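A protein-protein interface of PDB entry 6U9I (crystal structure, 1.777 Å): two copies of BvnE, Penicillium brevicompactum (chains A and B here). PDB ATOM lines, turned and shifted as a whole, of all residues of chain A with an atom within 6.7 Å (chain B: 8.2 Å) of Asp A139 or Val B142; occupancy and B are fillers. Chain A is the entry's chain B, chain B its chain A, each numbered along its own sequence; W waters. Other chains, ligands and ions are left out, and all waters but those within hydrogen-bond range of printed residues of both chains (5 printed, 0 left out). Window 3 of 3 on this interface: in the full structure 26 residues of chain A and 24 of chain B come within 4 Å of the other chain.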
ATOM      1  N   LEU A  54     -16.517  25.259   4.899  1.00  0.00           N
ATOM      2  CA  LEU A  54     -16.262  26.190   5.998  1.00  0.00           C
ATOM      3  C   LEU A  54     -17.560  26.711   6.608  1.00  0.00           C
ATOM      4  O   LEU A  54     -17.583  27.103   7.780  1.00  0.00           O
ATOM      5  CB  LEU A  54     -15.419  27.359   5.508  1.00  0.00           C
ATOM      6  CG  LEU A  54     -13.937  27.089   5.221  1.00  0.00           C
ATOM      7  CD1 LEU A  54     -13.334  28.339   4.614  1.00  0.00           C
ATOM      8  CD2 LEU A  54     -13.190  26.689   6.487  1.00  0.00           C
ATOM      9  N   ASN A 114      -2.083  32.066   5.786  1.00  0.00           N
ATOM     10  CA  ASN A 114      -2.973  31.250   4.973  1.00  0.00           C
ATOM     11  C   ASN A 114      -2.667  31.456   3.496  1.00  0.00           C
ATOM     12  O   ASN A 114      -1.840  32.287   3.113  1.00  0.00           O
ATOM     13  CB  ASN A 114      -4.447  31.552   5.281  1.00  0.00           C
ATOM     14  CG  ASN A 114      -5.300  30.305   5.223  1.00  0.00           C
ATOM     15  OD1 ASN A 114      -4.808  29.243   4.840  1.00  0.00           O
ATOM     16  ND2 ASN A 114      -6.557  30.408   5.628  1.00  0.00           N
ATOM     17  N   ALA A 136     -10.129  29.820   0.550  1.00  0.00           N
ATOM     18  CA  ALA A 136      -9.049  29.697   1.525  1.00  0.00           C
ATOM     19  C   ALA A 136      -8.593  28.252   1.685  1.00  0.00           C
ATOM     20  O   ALA A 136      -9.278  27.304   1.295  1.00  0.00           O
ATOM     21  CB  ALA A 136      -9.502  30.232   2.886  1.00  0.00           C
ATOM     22  N   ASP A 137      -7.409  28.094   2.273  1.00  0.00           N
ATOM     23  CA  ASP A 137      -6.944  26.795   2.766  1.00  0.00           C
ATOM     24  C   ASP A 137      -7.789  26.463   3.991  1.00  0.00           C
ATOM     25  O   ASP A 137      -7.621  27.061   5.061  1.00  0.00           O
ATOM     26  CB  ASP A 137      -5.444  26.894   3.058  1.00  0.00           C
ATOM     27  CG  ASP A 137      -4.856  25.685   3.789  1.00  0.00           C
ATOM     28  OD1 ASP A 137      -5.567  24.797   4.292  1.00  0.00           O
ATOM     29  OD2 ASP A 137      -3.612  25.646   3.866  1.00  0.00           O
ATOM     30  N   SER A 138      -8.752  25.551   3.821  1.00  0.00           N
ATOM     31  CA  SER A 138      -9.759  25.346   4.861  1.00  0.00           C
ATOM     32  C   SER A 138      -9.186  24.592   6.054  1.00  0.00           C
ATOM     33  O   SER A 138      -9.604  24.840   7.193  1.00  0.00           O
ATOM     34  CB  SER A 138     -10.965  24.588   4.295  1.00  0.00           C
ATOM     35  OG  SER A 138     -10.526  23.419   3.613  1.00  0.00           O
ATOM     36  N   ASP A 139      -8.240  23.670   5.817  1.00  0.00           N
ATOM     37  CA  ASP A 139      -7.550  23.011   6.926  1.00  0.00           C
ATOM     38  C   ASP A 139      -6.962  24.041   7.876  1.00  0.00           C
ATOM     39  O   ASP A 139      -7.082  23.912   9.104  1.00  0.00           O
ATOM     40  CB  ASP A 139      -6.453  22.075   6.395  1.00  0.00           C
ATOM     41  CG  ASP A 139      -5.650  21.402   7.507  1.00  0.00           C
ATOM     42  OD1 ASP A 139      -6.248  20.693   8.345  1.00  0.00           O
ATOM     43  OD2 ASP A 139      -4.414  21.567   7.530  1.00  0.00           O
ATOM     44  N   TYR A 140      -6.366  25.103   7.329  1.00  0.00           N
ATOM     45  CA  TYR A 140      -5.761  26.115   8.187  1.00  0.00           C
ATOM     46  C   TYR A 140      -6.816  26.918   8.933  1.00  0.00           C
ATOM     47  O   TYR A 140      -6.631  27.241  10.111  1.00  0.00           O
ATOM     48  CB  TYR A 140      -4.866  27.054   7.382  1.00  0.00           C
ATOM     49  CG  TYR A 140      -4.047  27.942   8.292  1.00  0.00           C
ATOM     50  CD1 TYR A 140      -2.800  27.524   8.758  1.00  0.00           C
ATOM     51  CD2 TYR A 140      -4.535  29.175   8.725  1.00  0.00           C
ATOM     52  CE1 TYR A 140      -2.054  28.318   9.617  1.00  0.00           C
ATOM     53  CE2 TYR A 140      -3.787  29.985   9.587  1.00  0.00           C
ATOM     54  CZ  TYR A 140      -2.547  29.546  10.025  1.00  0.00           C
ATOM     55  OH  TYR A 140      -1.794  30.329  10.871  1.00  0.00           O
ATOM     56  N   CYS A 141      -7.916  27.273   8.263  1.00  0.00           N
ATOM     57  CA  CYS A 141      -9.014  27.940   8.959  1.00  0.00           C
ATOM     58  C   CYS A 141      -9.493  27.114  10.143  1.00  0.00           C
ATOM     59  O   CYS A 141      -9.687  27.637  11.242  1.00  0.00           O
ATOM     60  CB  CYS A 141     -10.175  28.215   7.998  1.00  0.00           C
ATOM     61  SG  CYS A 141      -9.783  29.327   6.652  1.00  0.00           S
ATOM     62  N   VAL A 142      -9.680  25.815   9.936  1.00  0.00           N
ATOM     63  CA  VAL A 142     -10.169  24.953  11.006  1.00  0.00           C
ATOM     64  C   VAL A 142      -9.161  24.911  12.149  1.00  0.00           C
ATOM     65  O   VAL A 142      -9.527  25.035  13.327  1.00  0.00           O
ATOM     66  CB  VAL A 142     -10.480  23.555  10.441  1.00  0.00           C
ATOM     67  CG1 VAL A 142     -10.726  22.572  11.569  1.00  0.00           C
ATOM     68  CG2 VAL A 142     -11.681  23.629   9.498  1.00  0.00           C
ATOM     69  N   LYS A 143      -7.873  24.781  11.819  1.00  0.00           N
ATOM     70  CA  LYS A 143      -6.845  24.737  12.852  1.00  0.00           C
ATOM     71  C   LYS A 143      -6.780  26.048  13.619  1.00  0.00           C
ATOM     72  O   LYS A 143      -6.617  26.049  14.845  1.00  0.00           O
ATOM     73  CB  LYS A 143      -5.489  24.414  12.226  1.00  0.00           C
ATOM     74  CG  LYS A 143      -5.315  22.954  11.840  1.00  0.00           C
ATOM     75  CD  LYS A 143      -3.970  22.735  11.160  1.00  0.00           C
ATOM     76  CE  LYS A 143      -3.566  21.267  11.155  1.00  0.00           C
ATOM     77  NZ  LYS A 143      -4.662  20.391  10.654  1.00  0.00           N
ATOM     78  N   PHE A 144      -6.915  27.177  12.917  1.00  0.00           N
ATOM     79  CA  PHE A 144      -6.898  28.468  13.593  1.00  0.00           C
ATOM     80  C   PHE A 144      -8.070  28.612  14.556  1.00  0.00           C
ATOM     81  O   PHE A 144      -7.919  29.176  15.645  1.00  0.00           O
ATOM     82  CB  PHE A 144      -6.914  29.604  12.576  1.00  0.00           C
ATOM     83  CG  PHE A 144      -6.675  30.948  13.191  1.00  0.00           C
ATOM     84  CD1 PHE A 144      -5.419  31.279  13.679  1.00  0.00           C
ATOM     85  CD2 PHE A 144      -7.701  31.871  13.302  1.00  0.00           C
ATOM     86  CE1 PHE A 144      -5.187  32.516  14.259  1.00  0.00           C
ATOM     87  CE2 PHE A 144      -7.479  33.107  13.881  1.00  0.00           C
ATOM     88  CZ  PHE A 144      -6.221  33.430  14.361  1.00  0.00           C
ATOM     89  N   PRO B  51      -3.573  23.701  -1.499  1.00  0.00           N
ATOM     90  CA  PRO B  51      -2.540  24.620  -1.010  1.00  0.00           C
ATOM     91  C   PRO B  51      -1.272  23.899  -0.567  1.00  0.00           C
ATOM     92  O   PRO B  51      -1.267  22.671  -0.467  1.00  0.00           O
ATOM     93  CB  PRO B  51      -3.219  25.307   0.183  1.00  0.00           C
ATOM     94  CG  PRO B  51      -4.210  24.300   0.679  1.00  0.00           C
ATOM     95  CD  PRO B  51      -4.737  23.651  -0.593  1.00  0.00           C
ATOM     96  N   SER B  53       0.018  23.614   2.251  1.00  0.00           N
ATOM     97  CA  SER B  53      -0.097  22.920   3.528  1.00  0.00           C
ATOM     98  C   SER B  53      -0.413  21.433   3.373  1.00  0.00           C
ATOM     99  O   SER B  53      -0.135  20.654   4.289  1.00  0.00           O
ATOM    100  CB  SER B  53      -1.161  23.593   4.388  1.00  0.00           C
ATOM    101  OG  SER B  53      -2.451  23.404   3.828  1.00  0.00           O
ATOM    102  N   LEU B  54      -0.988  21.011   2.243  1.00  0.00           N
ATOM    103  CA  LEU B  54      -1.218  19.586   2.039  1.00  0.00           C
ATOM    104  C   LEU B  54       0.084  18.814   1.881  1.00  0.00           C
ATOM    105  O   LEU B  54       0.092  17.595   2.091  1.00  0.00           O
ATOM    106  CB  LEU B  54      -2.094  19.353   0.809  1.00  0.00           C
ATOM    107  CG  LEU B  54      -3.542  19.783   1.002  1.00  0.00           C
ATOM    108  CD1 LEU B  54      -4.278  19.721  -0.327  1.00  0.00           C
ATOM    109  CD2 LEU B  54      -4.201  18.892   2.050  1.00  0.00           C
ATOM    110  N   PHE B  56       2.036  18.138  -0.816  1.00  0.00           N
ATOM    111  CA  PHE B  56       2.240  17.310  -1.999  1.00  0.00           C
ATOM    112  C   PHE B  56       3.032  18.056  -3.065  1.00  0.00           C
ATOM    113  O   PHE B  56       2.708  19.199  -3.404  1.00  0.00           O
ATOM    114  CB  PHE B  56       0.892  16.858  -2.567  1.00  0.00           C
ATOM    115  CG  PHE B  56       0.117  15.974  -1.633  1.00  0.00           C
ATOM    116  CD1 PHE B  56       0.582  14.709  -1.314  1.00  0.00           C
ATOM    117  CD2 PHE B  56      -1.073  16.409  -1.070  1.00  0.00           C
ATOM    118  CE1 PHE B  56      -0.129  13.889  -0.449  1.00  0.00           C
ATOM    119  CE2 PHE B  56      -1.787  15.595  -0.203  1.00  0.00           C
ATOM    120  CZ  PHE B  56      -1.313  14.335   0.107  1.00  0.00           C
ATOM    121  N   TYR B 112     -17.343  10.614  -1.227  1.00  0.00           N
ATOM    122  CA  TYR B 112     -16.259  11.576  -1.389  1.00  0.00           C
ATOM    123  C   TYR B 112     -16.837  12.785  -2.110  1.00  0.00           C
ATOM    124  O   TYR B 112     -17.308  12.658  -3.244  1.00  0.00           O
ATOM    125  CB  TYR B 112     -15.106  10.969  -2.183  1.00  0.00           C
ATOM    126  CG  TYR B 112     -14.019  11.958  -2.537  1.00  0.00           C
ATOM    127  CD1 TYR B 112     -13.044  12.307  -1.610  1.00  0.00           C
ATOM    128  CD2 TYR B 112     -13.963  12.540  -3.799  1.00  0.00           C
ATOM    129  CE1 TYR B 112     -12.039  13.207  -1.926  1.00  0.00           C
ATOM    130  CE2 TYR B 112     -12.964  13.443  -4.126  1.00  0.00           C
ATOM    131  CZ  TYR B 112     -12.009  13.777  -3.184  1.00  0.00           C
ATOM    132  OH  TYR B 112     -11.012  14.675  -3.503  1.00  0.00           O
ATOM    133  N   ASN B 114     -15.715  16.621  -2.710  1.00  0.00           N
ATOM    134  CA  ASN B 114     -14.719  17.670  -2.543  1.00  0.00           C
ATOM    135  C   ASN B 114     -15.047  18.855  -3.445  1.00  0.00           C
ATOM    136  O   ASN B 114     -15.979  18.827  -4.256  1.00  0.00           O
ATOM    137  CB  ASN B 114     -13.308  17.132  -2.831  1.00  0.00           C
ATOM    138  CG  ASN B 114     -12.228  17.756  -1.937  1.00  0.00           C
ATOM    139  OD1 ASN B 114     -12.363  18.880  -1.461  1.00  0.00           O
ATOM    140  ND2 ASN B 114     -11.141  17.019  -1.720  1.00  0.00           N
ATOM    141  N   ALA B 136      -7.436  22.391  -3.612  1.00  0.00           N
ATOM    142  CA  ALA B 136      -8.499  21.600  -3.005  1.00  0.00           C
ATOM    143  C   ALA B 136      -8.994  22.220  -1.699  1.00  0.00           C
ATOM    144  O   ALA B 136      -8.344  23.081  -1.096  1.00  0.00           O
ATOM    145  CB  ALA B 136      -8.015  20.168  -2.735  1.00  0.00           C
ATOM    146  N   ASP B 137     -10.181  21.775  -1.281  1.00  0.00           N
ATOM    147  CA  ASP B 137     -10.678  21.949   0.086  1.00  0.00           C
ATOM    148  C   ASP B 137      -9.797  21.090   0.989  1.00  0.00           C
ATOM    149  O   ASP B 137      -9.969  19.870   1.067  1.00  0.00           O
ATOM    150  CB  ASP B 137     -12.148  21.533   0.142  1.00  0.00           C
ATOM    151  CG  ASP B 137     -12.782  21.669   1.533  1.00  0.00           C
ATOM    152  OD1 ASP B 137     -12.082  21.755   2.566  1.00  0.00           O
ATOM    153  OD2 ASP B 137     -14.026  21.654   1.590  1.00  0.00           O
ATOM    154  N   SER B 138      -8.818  21.714   1.647  1.00  0.00           N
ATOM    155  CA  SER B 138      -7.808  20.926   2.347  1.00  0.00           C
ATOM    156  C   SER B 138      -8.375  20.277   3.604  1.00  0.00           C
ATOM    157  O   SER B 138      -7.982  19.159   3.962  1.00  0.00           O
ATOM    158  CB  SER B 138      -6.612  21.813   2.691  1.00  0.00           C
ATOM    159  OG  SER B 138      -7.060  23.027   3.284  1.00  0.00           O
ATOM    160  N   ASP B 139      -9.281  20.968   4.305  1.00  0.00           N
ATOM    161  CA  ASP B 139      -9.930  20.336   5.452  1.00  0.00           C
ATOM    162  C   ASP B 139     -10.630  19.057   5.030  1.00  0.00           C
ATOM    163  O   ASP B 139     -10.529  18.029   5.712  1.00  0.00           O
ATOM    164  CB  ASP B 139     -10.934  21.282   6.114  1.00  0.00           C
ATOM    165  CG  ASP B 139     -11.674  20.624   7.279  1.00  0.00           C
ATOM    166  OD1 ASP B 139     -10.992  20.115   8.188  1.00  0.00           O
ATOM    167  OD2 ASP B 139     -12.927  20.601   7.282  1.00  0.00           O
ATOM    168  N   TYR B 140     -11.332  19.094   3.895  1.00  0.00           N
ATOM    169  CA  TYR B 140     -12.002  17.889   3.434  1.00  0.00           C
ATOM    170  C   TYR B 140     -10.989  16.808   3.087  1.00  0.00           C
ATOM    171  O   TYR B 140     -11.209  15.627   3.382  1.00  0.00           O
ATOM    172  CB  TYR B 140     -12.903  18.190   2.235  1.00  0.00           C
ATOM    173  CG  TYR B 140     -13.813  17.025   1.965  1.00  0.00           C
ATOM    174  CD1 TYR B 140     -15.024  16.911   2.618  1.00  0.00           C
ATOM    175  CD2 TYR B 140     -13.432  16.005   1.102  1.00  0.00           C
ATOM    176  CE1 TYR B 140     -15.851  15.829   2.400  1.00  0.00           C
ATOM    177  CE2 TYR B 140     -14.250  14.925   0.874  1.00  0.00           C
ATOM    178  CZ  TYR B 140     -15.462  14.841   1.528  1.00  0.00           C
ATOM    179  OH  TYR B 140     -16.285  13.761   1.313  1.00  0.00           O
ATOM    180  N   CYS B 141      -9.867  17.204   2.480  1.00  0.00           N
ATOM    181  CA  CYS B 141      -8.804  16.265   2.130  1.00  0.00           C
ATOM    182  C   CYS B 141      -8.295  15.528   3.364  1.00  0.00           C
ATOM    183  O   CYS B 141      -8.126  14.301   3.356  1.00  0.00           O
ATOM    184  CB  CYS B 141      -7.661  17.040   1.476  1.00  0.00           C
ATOM    185  SG  CYS B 141      -7.957  17.344  -0.276  1.00  0.00           S
ATOM    186  N   VAL B 142      -8.016  16.280   4.426  1.00  0.00           N
ATOM    187  CA  VAL B 142      -7.483  15.711   5.657  1.00  0.00           C
ATOM    188  C   VAL B 142      -8.524  14.829   6.325  1.00  0.00           C
ATOM    189  O   VAL B 142      -8.221  13.717   6.777  1.00  0.00           O
ATOM    190  CB  VAL B 142      -7.015  16.839   6.593  1.00  0.00           C
ATOM    191  CG1 VAL B 142      -6.548  16.263   7.915  1.00  0.00           C
ATOM    192  CG2 VAL B 142      -5.901  17.655   5.938  1.00  0.00           C
ATOM    193  N   LYS B 143      -9.766  15.307   6.396  1.00  0.00           N
ATOM    194  CA  LYS B 143     -10.826  14.512   7.002  1.00  0.00           C
ATOM    195  C   LYS B 143     -11.079  13.234   6.213  1.00  0.00           C
ATOM    196  O   LYS B 143     -11.332  12.176   6.801  1.00  0.00           O
ATOM    197  CB  LYS B 143     -12.101  15.343   7.114  1.00  0.00           C
ATOM    198  CG  LYS B 143     -12.007  16.457   8.138  1.00  0.00           C
ATOM    199  CD  LYS B 143     -13.382  16.960   8.502  1.00  0.00           C
ATOM    200  CE  LYS B 143     -13.319  18.207   9.366  1.00  0.00           C
ATOM    201  NZ  LYS B 143     -12.052  18.326  10.139  1.00  0.00           N
ATOM    202  N   PHE B 144     -11.009  13.305   4.880  1.00  0.00           N
ATOM    203  CA  PHE B 144     -11.236  12.098   4.094  1.00  0.00           C
ATOM    204  C   PHE B 144     -10.107  11.090   4.287  1.00  0.00           C
ATOM    205  O   PHE B 144     -10.354   9.878   4.291  1.00  0.00           O
ATOM    206  CB  PHE B 144     -11.410  12.438   2.614  1.00  0.00           C
ATOM    207  CG  PHE B 144     -11.794  11.254   1.766  1.00  0.00           C
ATOM    208  CD1 PHE B 144     -13.115  10.832   1.698  1.00  0.00           C
ATOM    209  CD2 PHE B 144     -10.833  10.562   1.044  1.00  0.00           C
ATOM    210  CE1 PHE B 144     -13.474   9.740   0.923  1.00  0.00           C
ATOM    211  CE2 PHE B 144     -11.180   9.474   0.267  1.00  0.00           C
ATOM    212  CZ  PHE B 144     -12.502   9.059   0.206  1.00  0.00           C
ATOM    213  N   ALA B 145      -8.871  11.565   4.459  1.00  0.00           N
ATOM    214  CA  ALA B 145      -7.779  10.656   4.782  1.00  0.00           C
ATOM    215  C   ALA B 145      -8.032   9.952   6.109  1.00  0.00           C
ATOM    216  O   ALA B 145      -7.811   8.741   6.229  1.00  0.00           O
ATOM    217  CB  ALA B 145      -6.452  11.417   4.816  1.00  0.00           C
ATOM    218  N   GLU B 146      -8.511  10.696   7.112  1.00  0.00           N
ATOM    219  CA  GLU B 146      -8.889  10.095   8.390  1.00  0.00           C
ATOM    220  C   GLU B 146      -9.977   9.044   8.205  1.00  0.00           C
ATOM    221  O   GLU B 146      -9.859   7.920   8.712  1.00  0.00           O
ATOM    222  CB  GLU B 146      -9.360  11.183   9.360  1.00  0.00           C
ATOM    223  CG  GLU B 146      -8.325  12.251   9.678  1.00  0.00           C
ATOM    224  CD  GLU B 146      -8.935  13.478  10.352  1.00  0.00           C
ATOM    225  OE1 GLU B 146      -8.178  14.418  10.675  1.00  0.00           O
ATOM    226  OE2 GLU B 146     -10.170  13.503  10.554  1.00  0.00           O
ATOM    227  N   ARG B 147     -11.053   9.396   7.490  1.00  0.00           N
ATOM    228  CA  ARG B 147     -12.157   8.457   7.287  1.00  0.00           C
ATOM    229  C   ARG B 147     -11.702   7.183   6.590  1.00  0.00           C
ATOM    230  O   ARG B 147     -12.241   6.103   6.859  1.00  0.00           O
ATOM    231  CB  ARG B 147     -13.276   9.104   6.472  1.00  0.00           C
ATOM    232  CG  ARG B 147     -14.046  10.186   7.177  1.00  0.00           C
ATOM    233  CD  ARG B 147     -14.901  10.941   6.175  1.00  0.00           C
ATOM    234  NE  ARG B 147     -15.753  10.027   5.420  1.00  0.00           N
ATOM    235  CZ  ARG B 147     -16.294  10.309   4.240  1.00  0.00           C
ATOM    236  NH1 ARG B 147     -16.059  11.483   3.664  1.00  0.00           N
ATOM    237  NH2 ARG B 147     -17.058   9.414   3.631  1.00  0.00           N
ATOM    238  N   GLN B 148     -10.731   7.299   5.698  1.00  0.00           N
ATOM    239  CA  GLN B 148     -10.223   6.167   4.967  1.00  0.00           C
ATOM    240  C   GLN B 148      -9.369   5.306   5.871  1.00  0.00           C
ATOM    241  O   GLN B 148      -9.501   4.092   5.837  1.00  0.00           O
ATOM    242  CB  GLN B 148      -9.485   6.580   3.689  1.00  0.00           C
ATOM    243  CG  GLN B 148     -10.363   6.801   2.466  1.00  0.00           C
ATOM    244  CD  GLN B 148      -9.656   6.453   1.171  1.00  0.00           C
ATOM    245  OE1 GLN B 148      -8.499   6.831   0.977  1.00  0.00           O
ATOM    246  NE2 GLN B 148     -10.344   5.707   0.280  1.00  0.00           N
ATOM    247  N   ALA B 149      -8.509   5.911   6.663  1.00  0.00           N
ATOM    248  CA  ALA B 149      -7.679   5.178   7.611  1.00  0.00           C
ATOM    249  C   ALA B 149      -8.533   4.368   8.578  1.00  0.00           C
ATOM    250  O   ALA B 149      -8.228   3.204   8.862  1.00  0.00           O
ATOM    251  CB  ALA B 149      -6.787   6.149   8.373  1.00  0.00           C
HETATM  252  O   HOH W   1      -3.609  21.135   4.816  1.00  0.00           O
HETATM  253  O   HOH W   2      -0.661  26.510   2.442  1.00  0.00           O
HETATM  254  O   HOH W   3      -8.623  19.983   9.193  1.00  0.00           O
HETATM  255  O   HOH W   4      -3.254  23.927   6.969  1.00  0.00           O
HETATM  256  O   HOH W   5      -8.894  24.697   0.999  1.00  0.00           O
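Asp A137 touches Ser B138, and with the chains exchanged Ser A138 touches Asp B137. Ser A138 touches Asp B139, and with the chains exchanged Asp A139 touches Ser B138. Asp B139 touches its own counterpart, Asp A139. Asp A139 touches Val B142, and with the chains exchanged Val A142 touches Asp B139. Positions printed for both chains: 54, 114, 136, 137, 138, 139, 140, 141, 142, 143 and 144. Of the 10 pairs that touch across the chains among the printed residues, 8 have their exchanged pair printed and touching as well.
Hydrophobic or aromatic side chains of chain A within 4 Å of the printed part of chain B: Val A142. Of the 20 printed residues of chain B, 6 touch a printed residue of chain A. Printed residues of chain B that touch a printed residue of chain A: Pro B51, Ser B53, Asp B137, Ser B138, Asp B139 and Val B142. Among the printed residues, 10 pairs touch across the chains. Among the printed residues, no Asp or Glu carboxylate lies within 4 Å of a Lys or Arg side-chain nitrogen of the other chain.
CG of Asp A137 touches CG of Pro B51, at 3.5 Å. OD1 of Asp A139 touches CG2 of Val B142, at 3.9 Å. Asp B139 touches Val A142 (CG to CG2, 3.7 Å).
OD1 of Asp A137 sits at hydrogen-bond distance from N of Tyr A140, at 3.2 Å. The side-chain carboxylate of Asp B137 lies close to the backbone NH of Asp B139 (3.4 Å). The side-chain sulfur (SG) of Cys A141 is in hydrogen-bond range of the backbone carbonyl oxygen (O) of Asp A137, at 3.5 Å. NZ of Lys B143 is in salt-bridge range of OD1 of Asp B139 (2.9 Å). The side-chain amino group (NZ) of Lys A143 lies within salt-bridge range of the side-chain carboxylate (OD1) of Asp A139 (2.8 Å). OD1 of Asp B137 lies within hydrogen-bond range of N of Tyr B140.
Val B142 touches just one residue of chain A: Asp A139 (3.9 Å). Of the printed residues of chain B, Ser A138 touches Asp B137 (2.5 Å), Ser B138 (3.1 Å) and Asp B139 (2.8 Å). Of the printed residues of chain A, Ser B53 touches Asp A137 (2.5 Å). Printed residues of chain B within 4 Å of Val A142: Asp B139. Printed residues of chain A within 4 Å of Ser B138: Asp A137 (2.5 Å), Ser A138 (3.1 Å) and Asp A139 (2.9 Å). Of the printed residues of chain B, Asp A137 touches Pro B51 (3.5 Å), Ser B53 (2.5 Å) and Ser B138 (2.5 Å). Of the printed residues of chain A, Asp B139 touches Ser A138, Asp A139 and Val A142. The nearest residue of chain A that does not touch Val B142 is Lys A143 (5.3 Å). The nearest printed residue of chain A that does not touch Asp B137 is Asp A139 (5.4 Å).
Water W3 bridges the side-chain carboxylate of Asp B139 (2.6 Å) and the side-chain carboxylate of Asp A139 (2.6 Å). Water W5 lies within hydrogen-bond range of O of Ala A136 (2.7 Å), O of Ala B136 (2.7 Å), N of Ser A138 (3.0 Å) and N of Ser B138 (3.1 Å). Water W4 lies within hydrogen-bond range of OD2 of Asp A139 (2.7 Å), OG of Ser B53 (3.3 Å) and N of Tyr A140 (3.3 Å). Water W1 bridges OG of Ser B53 (2.7 Å) and OD2 of Asp A139 (2.9 Å). Water W2 lies within hydrogen-bond range of the backbone NH of Ser B53 (3.0 Å) and the side-chain carboxylate of Asp A137 (3.4 Å).
The backbone NH of Asp A139 lies within hydrogen-bond range of the side-chain hydroxyl of Ser B138. N of Asp A139 sits close to N of Asp B139 (3.3 Å). OG of Ser B53 is in hydrogen-bond range of OD2 of Asp A137, at 2.5 Å. The side-chain carboxylate (OD1) of Asp B137 sits at hydrogen-bond distance from the side-chain hydroxyl (OG) of Ser A138 (2.5 Å). The side-chain hydroxyl (OG) of Ser B138 lies within hydrogen-bond range of the backbone NH (N) of Ser A138 (3.1 Å). The backbone NH (N) of Asp B139 sits at hydrogen-bond distance from the side-chain hydroxyl (OG) of Ser A138 (2.8 Å). OD1 of Asp A137 is in hydrogen-bond range of OG of Ser B138.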
